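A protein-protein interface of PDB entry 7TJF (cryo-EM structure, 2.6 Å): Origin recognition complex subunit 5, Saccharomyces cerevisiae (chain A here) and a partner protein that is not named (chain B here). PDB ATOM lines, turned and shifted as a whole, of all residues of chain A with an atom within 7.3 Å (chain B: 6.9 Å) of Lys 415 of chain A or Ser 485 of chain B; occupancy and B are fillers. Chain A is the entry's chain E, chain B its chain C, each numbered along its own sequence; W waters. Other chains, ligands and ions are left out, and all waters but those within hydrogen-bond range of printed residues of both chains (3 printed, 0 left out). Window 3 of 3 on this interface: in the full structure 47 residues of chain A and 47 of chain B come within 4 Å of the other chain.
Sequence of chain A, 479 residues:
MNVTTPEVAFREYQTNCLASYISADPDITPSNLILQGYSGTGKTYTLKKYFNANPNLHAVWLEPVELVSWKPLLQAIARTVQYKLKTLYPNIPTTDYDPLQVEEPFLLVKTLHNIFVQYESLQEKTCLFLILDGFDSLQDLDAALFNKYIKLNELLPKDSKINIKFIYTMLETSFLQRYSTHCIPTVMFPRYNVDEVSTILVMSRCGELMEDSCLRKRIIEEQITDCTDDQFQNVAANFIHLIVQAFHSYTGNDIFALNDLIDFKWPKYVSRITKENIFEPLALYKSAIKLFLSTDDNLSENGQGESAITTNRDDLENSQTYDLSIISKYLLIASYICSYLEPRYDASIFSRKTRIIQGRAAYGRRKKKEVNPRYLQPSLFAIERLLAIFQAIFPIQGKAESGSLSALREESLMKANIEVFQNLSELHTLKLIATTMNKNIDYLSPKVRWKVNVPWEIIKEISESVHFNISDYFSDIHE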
ATOM      1  N   LEU A 387     -23.152  -6.683 -13.266  1.00  0.00           N
ATOM      2  CA  LEU A 387     -23.368  -6.453 -14.689  1.00  0.00           C
ATOM      3  C   LEU A 387     -24.854  -6.459 -15.041  1.00  0.00           C
ATOM      4  O   LEU A 387     -25.286  -5.695 -15.910  1.00  0.00           O
ATOM      5  CB  LEU A 387     -22.607  -7.495 -15.502  1.00  0.00           C
ATOM      6  CG  LEU A 387     -21.082  -7.442 -15.482  1.00  0.00           C
ATOM      7  CD1 LEU A 387     -20.519  -8.608 -16.266  1.00  0.00           C
ATOM      8  CD2 LEU A 387     -20.590  -6.123 -16.049  1.00  0.00           C
ATOM      9  N   PHE A 390     -26.164  -3.118 -13.782  1.00  0.00           N
ATOM     10  CA  PHE A 390     -25.597  -2.113 -14.680  1.00  0.00           C
ATOM     11  C   PHE A 390     -26.328  -2.087 -16.018  1.00  0.00           C
ATOM     12  O   PHE A 390     -26.568  -1.012 -16.576  1.00  0.00           O
ATOM     13  CB  PHE A 390     -24.104  -2.404 -14.874  1.00  0.00           C
ATOM     14  CG  PHE A 390     -23.453  -1.627 -15.988  1.00  0.00           C
ATOM     15  CD1 PHE A 390     -23.067  -0.312 -15.795  1.00  0.00           C
ATOM     16  CD2 PHE A 390     -23.195  -2.224 -17.217  1.00  0.00           C
ATOM     17  CE1 PHE A 390     -22.452   0.400 -16.806  1.00  0.00           C
ATOM     18  CE2 PHE A 390     -22.591  -1.512 -18.237  1.00  0.00           C
ATOM     19  CZ  PHE A 390     -22.217  -0.199 -18.029  1.00  0.00           C
ATOM     20  N   GLN A 391     -26.682  -3.264 -16.544  1.00  0.00           N
ATOM     21  CA  GLN A 391     -27.480  -3.346 -17.762  1.00  0.00           C
ATOM     22  C   GLN A 391     -28.881  -2.789 -17.535  1.00  0.00           C
ATOM     23  O   GLN A 391     -29.452  -2.136 -18.417  1.00  0.00           O
ATOM     24  CB  GLN A 391     -27.534  -4.799 -18.248  1.00  0.00           C
ATOM     25  CG  GLN A 391     -28.335  -5.015 -19.518  1.00  0.00           C
ATOM     26  CD  GLN A 391     -28.380  -6.464 -19.965  1.00  0.00           C
ATOM     27  OE1 GLN A 391     -28.932  -7.323 -19.282  1.00  0.00           O
ATOM     28  NE2 GLN A 391     -27.797  -6.740 -21.124  1.00  0.00           N
ATOM     29  N   GLU A 411     -31.692  -4.597 -31.102  1.00  0.00           N
ATOM     30  CA  GLU A 411     -31.514  -5.216 -29.781  1.00  0.00           C
ATOM     31  C   GLU A 411     -30.900  -4.223 -28.788  1.00  0.00           C
ATOM     32  O   GLU A 411     -29.778  -4.380 -28.305  1.00  0.00           O
ATOM     33  CB  GLU A 411     -30.691  -6.508 -29.872  1.00  0.00           C
ATOM     34  CG  GLU A 411     -31.382  -7.629 -30.634  1.00  0.00           C
ATOM     35  CD  GLU A 411     -30.515  -8.867 -30.768  1.00  0.00           C
ATOM     36  OE1 GLU A 411     -29.314  -8.794 -30.434  1.00  0.00           O
ATOM     37  OE2 GLU A 411     -31.036  -9.913 -31.211  1.00  0.00           O
ATOM     38  N   LEU A 413     -29.999  -3.039 -25.941  1.00  0.00           N
ATOM     39  CA  LEU A 413     -29.611  -3.304 -24.562  1.00  0.00           C
ATOM     40  C   LEU A 413     -28.106  -3.499 -24.563  1.00  0.00           C
ATOM     41  O   LEU A 413     -27.600  -4.352 -25.298  1.00  0.00           O
ATOM     42  CB  LEU A 413     -30.308  -4.549 -24.001  1.00  0.00           C
ATOM     43  CG  LEU A 413     -31.350  -4.327 -22.906  1.00  0.00           C
ATOM     44  CD1 LEU A 413     -31.880  -5.659 -22.392  1.00  0.00           C
ATOM     45  CD2 LEU A 413     -30.810  -3.465 -21.777  1.00  0.00           C
ATOM     46  N   MET A 414     -27.392  -2.715 -23.760  1.00  0.00           N
ATOM     47  CA  MET A 414     -25.939  -2.765 -23.803  1.00  0.00           C
ATOM     48  C   MET A 414     -25.425  -4.003 -23.084  1.00  0.00           C
ATOM     49  O   MET A 414     -25.770  -4.256 -21.926  1.00  0.00           O
ATOM     50  CB  MET A 414     -25.324  -1.504 -23.203  1.00  0.00           C
ATOM     51  CG  MET A 414     -24.183  -0.968 -24.054  1.00  0.00           C
ATOM     52  SD  MET A 414     -23.230   0.354 -23.302  1.00  0.00           S
ATOM     53  CE  MET A 414     -21.836  -0.546 -22.647  1.00  0.00           C
ATOM     54  N   LYS A 415     -24.610  -4.777 -23.786  1.00  0.00           N
ATOM     55  CA  LYS A 415     -23.983  -5.969 -23.244  1.00  0.00           C
ATOM     56  C   LYS A 415     -22.590  -5.624 -22.737  1.00  0.00           C
ATOM     57  O   LYS A 415     -21.960  -4.671 -23.198  1.00  0.00           O
ATOM     58  CB  LYS A 415     -23.906  -7.067 -24.304  1.00  0.00           C
ATOM     59  CG  LYS A 415     -25.271  -7.575 -24.762  1.00  0.00           C
ATOM     60  CD  LYS A 415     -25.181  -8.931 -25.454  1.00  0.00           C
ATOM     61  CE  LYS A 415     -25.169  -8.827 -26.979  1.00  0.00           C
ATOM     62  NZ  LYS A 415     -24.304  -7.744 -27.530  1.00  0.00           N
ATOM     63  N   ALA A 416     -22.125  -6.400 -21.764  1.00  0.00           N
ATOM     64  CA  ALA A 416     -20.812  -6.173 -21.169  1.00  0.00           C
ATOM     65  C   ALA A 416     -19.742  -6.620 -22.156  1.00  0.00           C
ATOM     66  O   ALA A 416     -19.359  -7.791 -22.194  1.00  0.00           O
ATOM     67  CB  ALA A 416     -20.691  -6.918 -19.846  1.00  0.00           C
ATOM     68  N   ASN A 417     -19.262  -5.681 -22.965  1.00  0.00           N
ATOM     69  CA  ASN A 417     -18.165  -5.928 -23.886  1.00  0.00           C
ATOM     70  C   ASN A 417     -16.847  -5.699 -23.146  1.00  0.00           C
ATOM     71  O   ASN A 417     -16.821  -5.575 -21.919  1.00  0.00           O
ATOM     72  CB  ASN A 417     -18.318  -5.056 -25.130  1.00  0.00           C
ATOM     73  CG  ASN A 417     -18.117  -3.584 -24.843  1.00  0.00           C
ATOM     74  OD1 ASN A 417     -18.508  -3.084 -23.790  1.00  0.00           O
ATOM     75  ND2 ASN A 417     -17.510  -2.878 -25.787  1.00  0.00           N
ATOM     76  N   ILE A 418     -15.731  -5.640 -23.878  1.00  0.00           N
ATOM     77  CA  ILE A 418     -14.431  -5.507 -23.226  1.00  0.00           C
ATOM     78  C   ILE A 418     -14.233  -4.115 -22.639  1.00  0.00           C
ATOM     79  O   ILE A 418     -13.394  -3.940 -21.750  1.00  0.00           O
ATOM     80  CB  ILE A 418     -13.294  -5.910 -24.202  1.00  0.00           C
ATOM     81  CG1 ILE A 418     -13.208  -5.027 -25.461  1.00  0.00           C
ATOM     82  CG2 ILE A 418     -13.449  -7.360 -24.622  1.00  0.00           C
ATOM     83  CD1 ILE A 418     -12.306  -3.784 -25.410  1.00  0.00           C
ATOM     84  N   GLU A 419     -14.971  -3.116 -23.128  1.00  0.00           N
ATOM     85  CA  GLU A 419     -14.879  -1.776 -22.559  1.00  0.00           C
ATOM     86  C   GLU A 419     -15.459  -1.733 -21.151  1.00  0.00           C
ATOM     87  O   GLU A 419     -14.922  -1.046 -20.276  1.00  0.00           O
ATOM     88  CB  GLU A 419     -15.583  -0.772 -23.468  1.00  0.00           C
ATOM     89  CG  GLU A 419     -15.006  -0.712 -24.866  1.00  0.00           C
ATOM     90  CD  GLU A 419     -15.641   0.369 -25.719  1.00  0.00           C
ATOM     91  OE1 GLU A 419     -16.665   0.085 -26.374  1.00  0.00           O
ATOM     92  OE2 GLU A 419     -15.110   1.499 -25.740  1.00  0.00           O
ATOM     93  N   VAL A 420     -16.539  -2.479 -20.915  1.00  0.00           N
ATOM     94  CA  VAL A 420     -17.147  -2.550 -19.588  1.00  0.00           C
ATOM     95  C   VAL A 420     -16.206  -3.230 -18.600  1.00  0.00           C
ATOM     96  O   VAL A 420     -16.010  -2.748 -17.477  1.00  0.00           O
ATOM     97  CB  VAL A 420     -18.505  -3.270 -19.679  1.00  0.00           C
ATOM     98  CG1 VAL A 420     -19.126  -3.450 -18.301  1.00  0.00           C
ATOM     99  CG2 VAL A 420     -19.439  -2.500 -20.582  1.00  0.00           C
ATOM    100  N   PHE A 421     -15.582  -4.336 -19.015  1.00  0.00           N
ATOM    101  CA  PHE A 421     -14.640  -5.036 -18.149  1.00  0.00           C
ATOM    102  C   PHE A 421     -13.368  -4.229 -17.924  1.00  0.00           C
ATOM    103  O   PHE A 421     -12.810  -4.258 -16.822  1.00  0.00           O
ATOM    104  CB  PHE A 421     -14.314  -6.409 -18.736  1.00  0.00           C
ATOM    105  CG  PHE A 421     -15.396  -7.423 -18.517  1.00  0.00           C
ATOM    106  CD1 PHE A 421     -16.433  -7.555 -19.426  1.00  0.00           C
ATOM    107  CD2 PHE A 421     -15.391  -8.227 -17.390  1.00  0.00           C
ATOM    108  CE1 PHE A 421     -17.439  -8.482 -19.221  1.00  0.00           C
ATOM    109  CE2 PHE A 421     -16.391  -9.155 -17.178  1.00  0.00           C
ATOM    110  CZ  PHE A 421     -17.418  -9.283 -18.096  1.00  0.00           C
ATOM    111  N   SER B 482     -17.748  -7.900 -28.184  1.00  0.00           N
ATOM    112  CA  SER B 482     -18.628  -8.393 -27.127  1.00  0.00           C
ATOM    113  C   SER B 482     -18.194  -9.819 -26.807  1.00  0.00           C
ATOM    114  O   SER B 482     -18.778 -10.797 -27.274  1.00  0.00           O
ATOM    115  CB  SER B 482     -20.086  -8.322 -27.559  1.00  0.00           C
ATOM    116  OG  SER B 482     -20.311  -9.120 -28.705  1.00  0.00           O
ATOM    117  N   TYR B 483     -17.154  -9.911 -25.970  1.00  0.00           N
ATOM    118  CA  TYR B 483     -16.380 -11.136 -25.775  1.00  0.00           C
ATOM    119  C   TYR B 483     -17.235 -12.262 -25.195  1.00  0.00           C
ATOM    120  O   TYR B 483     -17.388 -13.329 -25.810  1.00  0.00           O
ATOM    121  CB  TYR B 483     -15.178 -10.803 -24.873  1.00  0.00           C
ATOM    122  CG  TYR B 483     -14.242 -11.928 -24.464  1.00  0.00           C
ATOM    123  CD1 TYR B 483     -14.511 -12.727 -23.352  1.00  0.00           C
ATOM    124  CD2 TYR B 483     -13.051 -12.143 -25.147  1.00  0.00           C
ATOM    125  CE1 TYR B 483     -13.653 -13.735 -22.970  1.00  0.00           C
ATOM    126  CE2 TYR B 483     -12.178 -13.146 -24.763  1.00  0.00           C
ATOM    127  CZ  TYR B 483     -12.487 -13.941 -23.676  1.00  0.00           C
ATOM    128  OH  TYR B 483     -11.631 -14.943 -23.285  1.00  0.00           O
ATOM    129  N   LYS B 484     -17.821 -12.031 -24.015  1.00  0.00           N
ATOM    130  CA  LYS B 484     -18.627 -13.069 -23.385  1.00  0.00           C
ATOM    131  C   LYS B 484     -19.930 -13.298 -24.140  1.00  0.00           C
ATOM    132  O   LYS B 484     -20.436 -14.424 -24.160  1.00  0.00           O
ATOM    133  CB  LYS B 484     -18.876 -12.728 -21.908  1.00  0.00           C
ATOM    134  CG  LYS B 484     -20.031 -11.798 -21.592  1.00  0.00           C
ATOM    135  CD  LYS B 484     -20.082 -11.483 -20.104  1.00  0.00           C
ATOM    136  CE  LYS B 484     -20.970 -12.461 -19.356  1.00  0.00           C
ATOM    137  NZ  LYS B 484     -22.414 -12.263 -19.651  1.00  0.00           N
ATOM    138  N   SER B 485     -20.442 -12.267 -24.822  1.00  0.00           N
ATOM    139  CA  SER B 485     -21.627 -12.435 -25.654  1.00  0.00           C
ATOM    140  C   SER B 485     -21.321 -13.289 -26.878  1.00  0.00           C
ATOM    141  O   SER B 485     -22.151 -14.106 -27.288  1.00  0.00           O
ATOM    142  CB  SER B 485     -22.174 -11.069 -26.069  1.00  0.00           C
ATOM    143  OG  SER B 485     -22.737 -11.117 -27.366  1.00  0.00           O
ATOM    144  N   ASN B 486     -20.128 -13.122 -27.463  1.00  0.00           N
ATOM    145  CA  ASN B 486     -19.712 -13.975 -28.574  1.00  0.00           C
ATOM    146  C   ASN B 486     -19.532 -15.421 -28.131  1.00  0.00           C
ATOM    147  O   ASN B 486     -19.901 -16.344 -28.868  1.00  0.00           O
ATOM    148  CB  ASN B 486     -18.422 -13.449 -29.203  1.00  0.00           C
ATOM    149  CG  ASN B 486     -18.640 -12.187 -30.013  1.00  0.00           C
ATOM    150  OD1 ASN B 486     -19.728 -11.949 -30.533  1.00  0.00           O
ATOM    151  ND2 ASN B 486     -17.605 -11.367 -30.114  1.00  0.00           N
ATOM    152  N   ILE B 487     -18.978 -15.634 -26.930  1.00  0.00           N
ATOM    153  CA  ILE B 487     -18.837 -16.992 -26.402  1.00  0.00           C
ATOM    154  C   ILE B 487     -20.206 -17.630 -26.172  1.00  0.00           C
ATOM    155  O   ILE B 487     -20.437 -18.789 -26.548  1.00  0.00           O
ATOM    156  CB  ILE B 487     -17.994 -16.984 -25.112  1.00  0.00           C
ATOM    157  CG1 ILE B 487     -16.585 -16.466 -25.394  1.00  0.00           C
ATOM    158  CG2 ILE B 487     -17.915 -18.381 -24.504  1.00  0.00           C
ATOM    159  CD1 ILE B 487     -15.814 -17.316 -26.348  1.00  0.00           C
ATOM    160  N   GLU B 488     -21.142 -16.867 -25.586  1.00  0.00           N
ATOM    161  CA  GLU B 488     -22.495 -17.367 -25.344  1.00  0.00           C
ATOM    162  C   GLU B 488     -23.222 -17.688 -26.645  1.00  0.00           C
ATOM    163  O   GLU B 488     -23.900 -18.717 -26.745  1.00  0.00           O
ATOM    164  CB  GLU B 488     -23.314 -16.348 -24.544  1.00  0.00           C
ATOM    165  CG  GLU B 488     -23.005 -16.075 -23.045  1.00  0.00           C
ATOM    166  CD  GLU B 488     -23.016 -17.280 -22.096  1.00  0.00           C
ATOM    167  OE1 GLU B 488     -22.333 -18.302 -22.325  1.00  0.00           O
ATOM    168  OE2 GLU B 488     -23.765 -17.204 -21.101  1.00  0.00           O
ATOM    169  N   ASP B 489     -23.094 -16.821 -27.651  1.00  0.00           N
ATOM    170  CA  ASP B 489     -23.795 -17.039 -28.910  1.00  0.00           C
ATOM    171  C   ASP B 489     -23.164 -18.150 -29.738  1.00  0.00           C
ATOM    172  O   ASP B 489     -23.869 -18.814 -30.504  1.00  0.00           O
ATOM    173  CB  ASP B 489     -23.848 -15.739 -29.713  1.00  0.00           C
ATOM    174  CG  ASP B 489     -24.731 -14.687 -29.064  1.00  0.00           C
ATOM    175  OD1 ASP B 489     -25.235 -14.936 -27.948  1.00  0.00           O
ATOM    176  OD2 ASP B 489     -24.927 -13.611 -29.666  1.00  0.00           O
ATOM    177  N   ASN B 490     -21.852 -18.372 -29.610  1.00  0.00           N
ATOM    178  CA  ASN B 490     -21.245 -19.522 -30.269  1.00  0.00           C
ATOM    179  C   ASN B 490     -21.615 -20.822 -29.569  1.00  0.00           C
ATOM    180  O   ASN B 490     -21.734 -21.862 -30.226  1.00  0.00           O
ATOM    181  CB  ASN B 490     -19.724 -19.363 -30.333  1.00  0.00           C
ATOM    182  CG  ASN B 490     -19.295 -18.264 -31.283  1.00  0.00           C
ATOM    183  OD1 ASN B 490     -20.018 -17.915 -32.212  1.00  0.00           O
ATOM    184  ND2 ASN B 490     -18.111 -17.715 -31.055  1.00  0.00           N
ATOM    185  N   LEU B 491     -21.795 -20.787 -28.246  1.00  0.00           N
ATOM    186  CA  LEU B 491     -22.227 -21.984 -27.530  1.00  0.00           C
ATOM    187  C   LEU B 491     -23.681 -22.327 -27.831  1.00  0.00           C
ATOM    188  O   LEU B 491     -24.014 -23.497 -28.045  1.00  0.00           O
ATOM    189  CB  LEU B 491     -22.030 -21.798 -26.027  1.00  0.00           C
ATOM    190  CG  LEU B 491     -20.626 -22.087 -25.505  1.00  0.00           C
ATOM    191  CD1 LEU B 491     -20.479 -21.591 -24.073  1.00  0.00           C
ATOM    192  CD2 LEU B 491     -20.327 -23.572 -25.610  1.00  0.00           C
ATOM    193  N   ARG B 614     -26.625 -15.368 -20.701  1.00  0.00           N
ATOM    194  CA  ARG B 614     -26.513 -14.821 -22.047  1.00  0.00           C
ATOM    195  C   ARG B 614     -27.243 -13.484 -22.139  1.00  0.00           C
ATOM    196  O   ARG B 614     -28.351 -13.335 -21.619  1.00  0.00           O
ATOM    197  CB  ARG B 614     -27.076 -15.821 -23.059  1.00  0.00           C
ATOM    198  CG  ARG B 614     -27.401 -15.251 -24.430  1.00  0.00           C
ATOM    199  CD  ARG B 614     -27.417 -16.323 -25.495  1.00  0.00           C
ATOM    200  NE  ARG B 614     -27.511 -15.749 -26.832  1.00  0.00           N
ATOM    201  CZ  ARG B 614     -28.650 -15.497 -27.463  1.00  0.00           C
ATOM    202  NH1 ARG B 614     -29.820 -15.762 -26.907  1.00  0.00           N
ATOM    203  NH2 ARG B 614     -28.614 -14.965 -28.680  1.00  0.00           N
ATOM    204  N   GLY B 615     -26.611 -12.504 -22.780  1.00  0.00           N
ATOM    205  CA  GLY B 615     -27.239 -11.220 -23.001  1.00  0.00           C
ATOM    206  C   GLY B 615     -27.069 -10.215 -21.888  1.00  0.00           C
ATOM    207  O   GLY B 615     -27.832  -9.245 -21.829  1.00  0.00           O
ATOM    208  N   ILE B 616     -26.100 -10.410 -21.003  1.00  0.00           N
ATOM    209  CA  ILE B 616     -25.876  -9.477 -19.910  1.00  0.00           C
ATOM    210  C   ILE B 616     -24.686  -8.576 -20.250  1.00  0.00           C
ATOM    211  O   ILE B 616     -24.755  -7.348 -20.138  1.00  0.00           O
ATOM    212  CB  ILE B 616     -25.681 -10.237 -18.577  1.00  0.00           C
ATOM    213  CG1 ILE B 616     -27.042 -10.584 -17.969  1.00  0.00           C
ATOM    214  CG2 ILE B 616     -24.865  -9.427 -17.596  1.00  0.00           C
ATOM    215  CD1 ILE B 616     -26.985 -11.140 -16.558  1.00  0.00           C
ATOM    216  OXT ILE B 616     -23.629  -9.047 -20.667  1.00  0.00           O
HETATM  217  O   HOH W   1     -23.998  -4.898 -19.709  1.00  0.00           O
HETATM  218  O   HOH W   2     -20.070  -9.334 -24.372  1.00  0.00           O
HETATM  219  O   HOH W   3     -16.899  -9.259 -22.908  1.00  0.00           O
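The side-chain amide nitrogen of Gln 391 of chain A lies within hydrogen-bond range of the backbone carbonyl oxygen of Gly 615 of chain B (2.6 Å).
The chain-end carboxylate (O) of Ile 616 of chain B sits at hydrogen-bond distance from the side-chain amide nitrogen (NE2) of Gln 391 of chain A (3.3 Å).
O of Ile 616 of chain B sits at hydrogen-bond distance from N of Ala 416 of chain A.
The side-chain hydroxyl (OG) of Ser 482 of chain B is in hydrogen-bond range of the side-chain hydroxyl (OG) of Ser 485 of chain B, at 3.4 Å.
ND2 of Asn 486 of chain B sits close to O of Ser 482 of chain B.
The chain-end carboxylate of Ile 616 of chain B lies within salt-bridge range of the side-chain amino group of Lys 484 of chain B (3.6 Å).
The backbone carbonyl oxygen (O) of Met 414 of chain A lies within hydrogen-bond range of the side-chain amide nitrogen (NE2) of Gln 391 of chain A.
The side-chain amide nitrogen (ND2) of Asn 417 of chain A lies within hydrogen-bond range of the side-chain carboxylate (OE1) of Glu 419 of chain A.
Among the printed residues, merely in contact across the chains: Leu 387 of chain A with Ile 616 of chain B, Met 414 of chain A with Ile 616 of chain B, Lys 415 of chain A with Ser 485 of chain B, Lys 415 of chain A with Gly 615 of chain B, Lys 415 of chain A with Ile 616 of chain B, Asn 417 of chain A with Ser 482 of chain B, Ile 418 of chain A with Tyr 483 of chain B and Phe 421 of chain A with Lys 484 of chain B.
Printed residues of chain B within 4 Å of Gln 391 of chain A: Gly 615 and Ile 616.
Of chain B, only Ser 485 (3.4 Å), Gly 615 (3.9 Å) and Ile 616 (3.5 Å) come within 4 Å of Lys 415 of chain A.
Of the printed residues of chain B, Ile 418 of chain A touches Tyr 483 (3.9 Å).
Of the printed residues of chain B, Phe 421 of chain A touches Lys 484 (3.996 Å).
Of the printed residues of chain A, Lys 484 of chain B touches Phe 421 (3.996 Å).
Ser 485 of chain B touches just one residue of chain A: Lys 415.
Of the printed residues of chain A, Gly 615 of chain B touches Gln 391 and Lys 415.
The nearest residue of chain A that does not touch Ser 485 of chain B is Ala 416 of chain A (5.3 Å).
Along chain B the printed residues that touch a printed residue of chain A span positions 482 to 616.
Of the 13 printed residues of chain A, 8 touch a printed residue of chain B.
Printed residues of chain A that touch a printed residue of chain B: Leu 387, Gln 391, Met 414, Lys 415, Ala 416, Asn 417, Ile 418 and Phe 421.
Among the printed residues, 11 pairs touch across the chains.
Water W1 lies within hydrogen-bond range of O of Ile 616 of chain B (2.6 Å), O of Met 414 of chain A (2.9 Å) and N of Ala 416 of chain A (3.2 Å).
Water W2 lies within hydrogen-bond range of O of Ala 416 of chain A (2.8 Å), N of Ser 485 of chain B (3.0 Å), N of Tyr 483 of chain B (3.4 Å) and O of Ser 482 of chain B (3.5 Å).
Water W3 lies within hydrogen-bond range of O of Ala 416 of chain A (3.0 Å), N of Lys 484 of chain B (3.1 Å) and N of Tyr 483 of chain B (3.1 Å).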
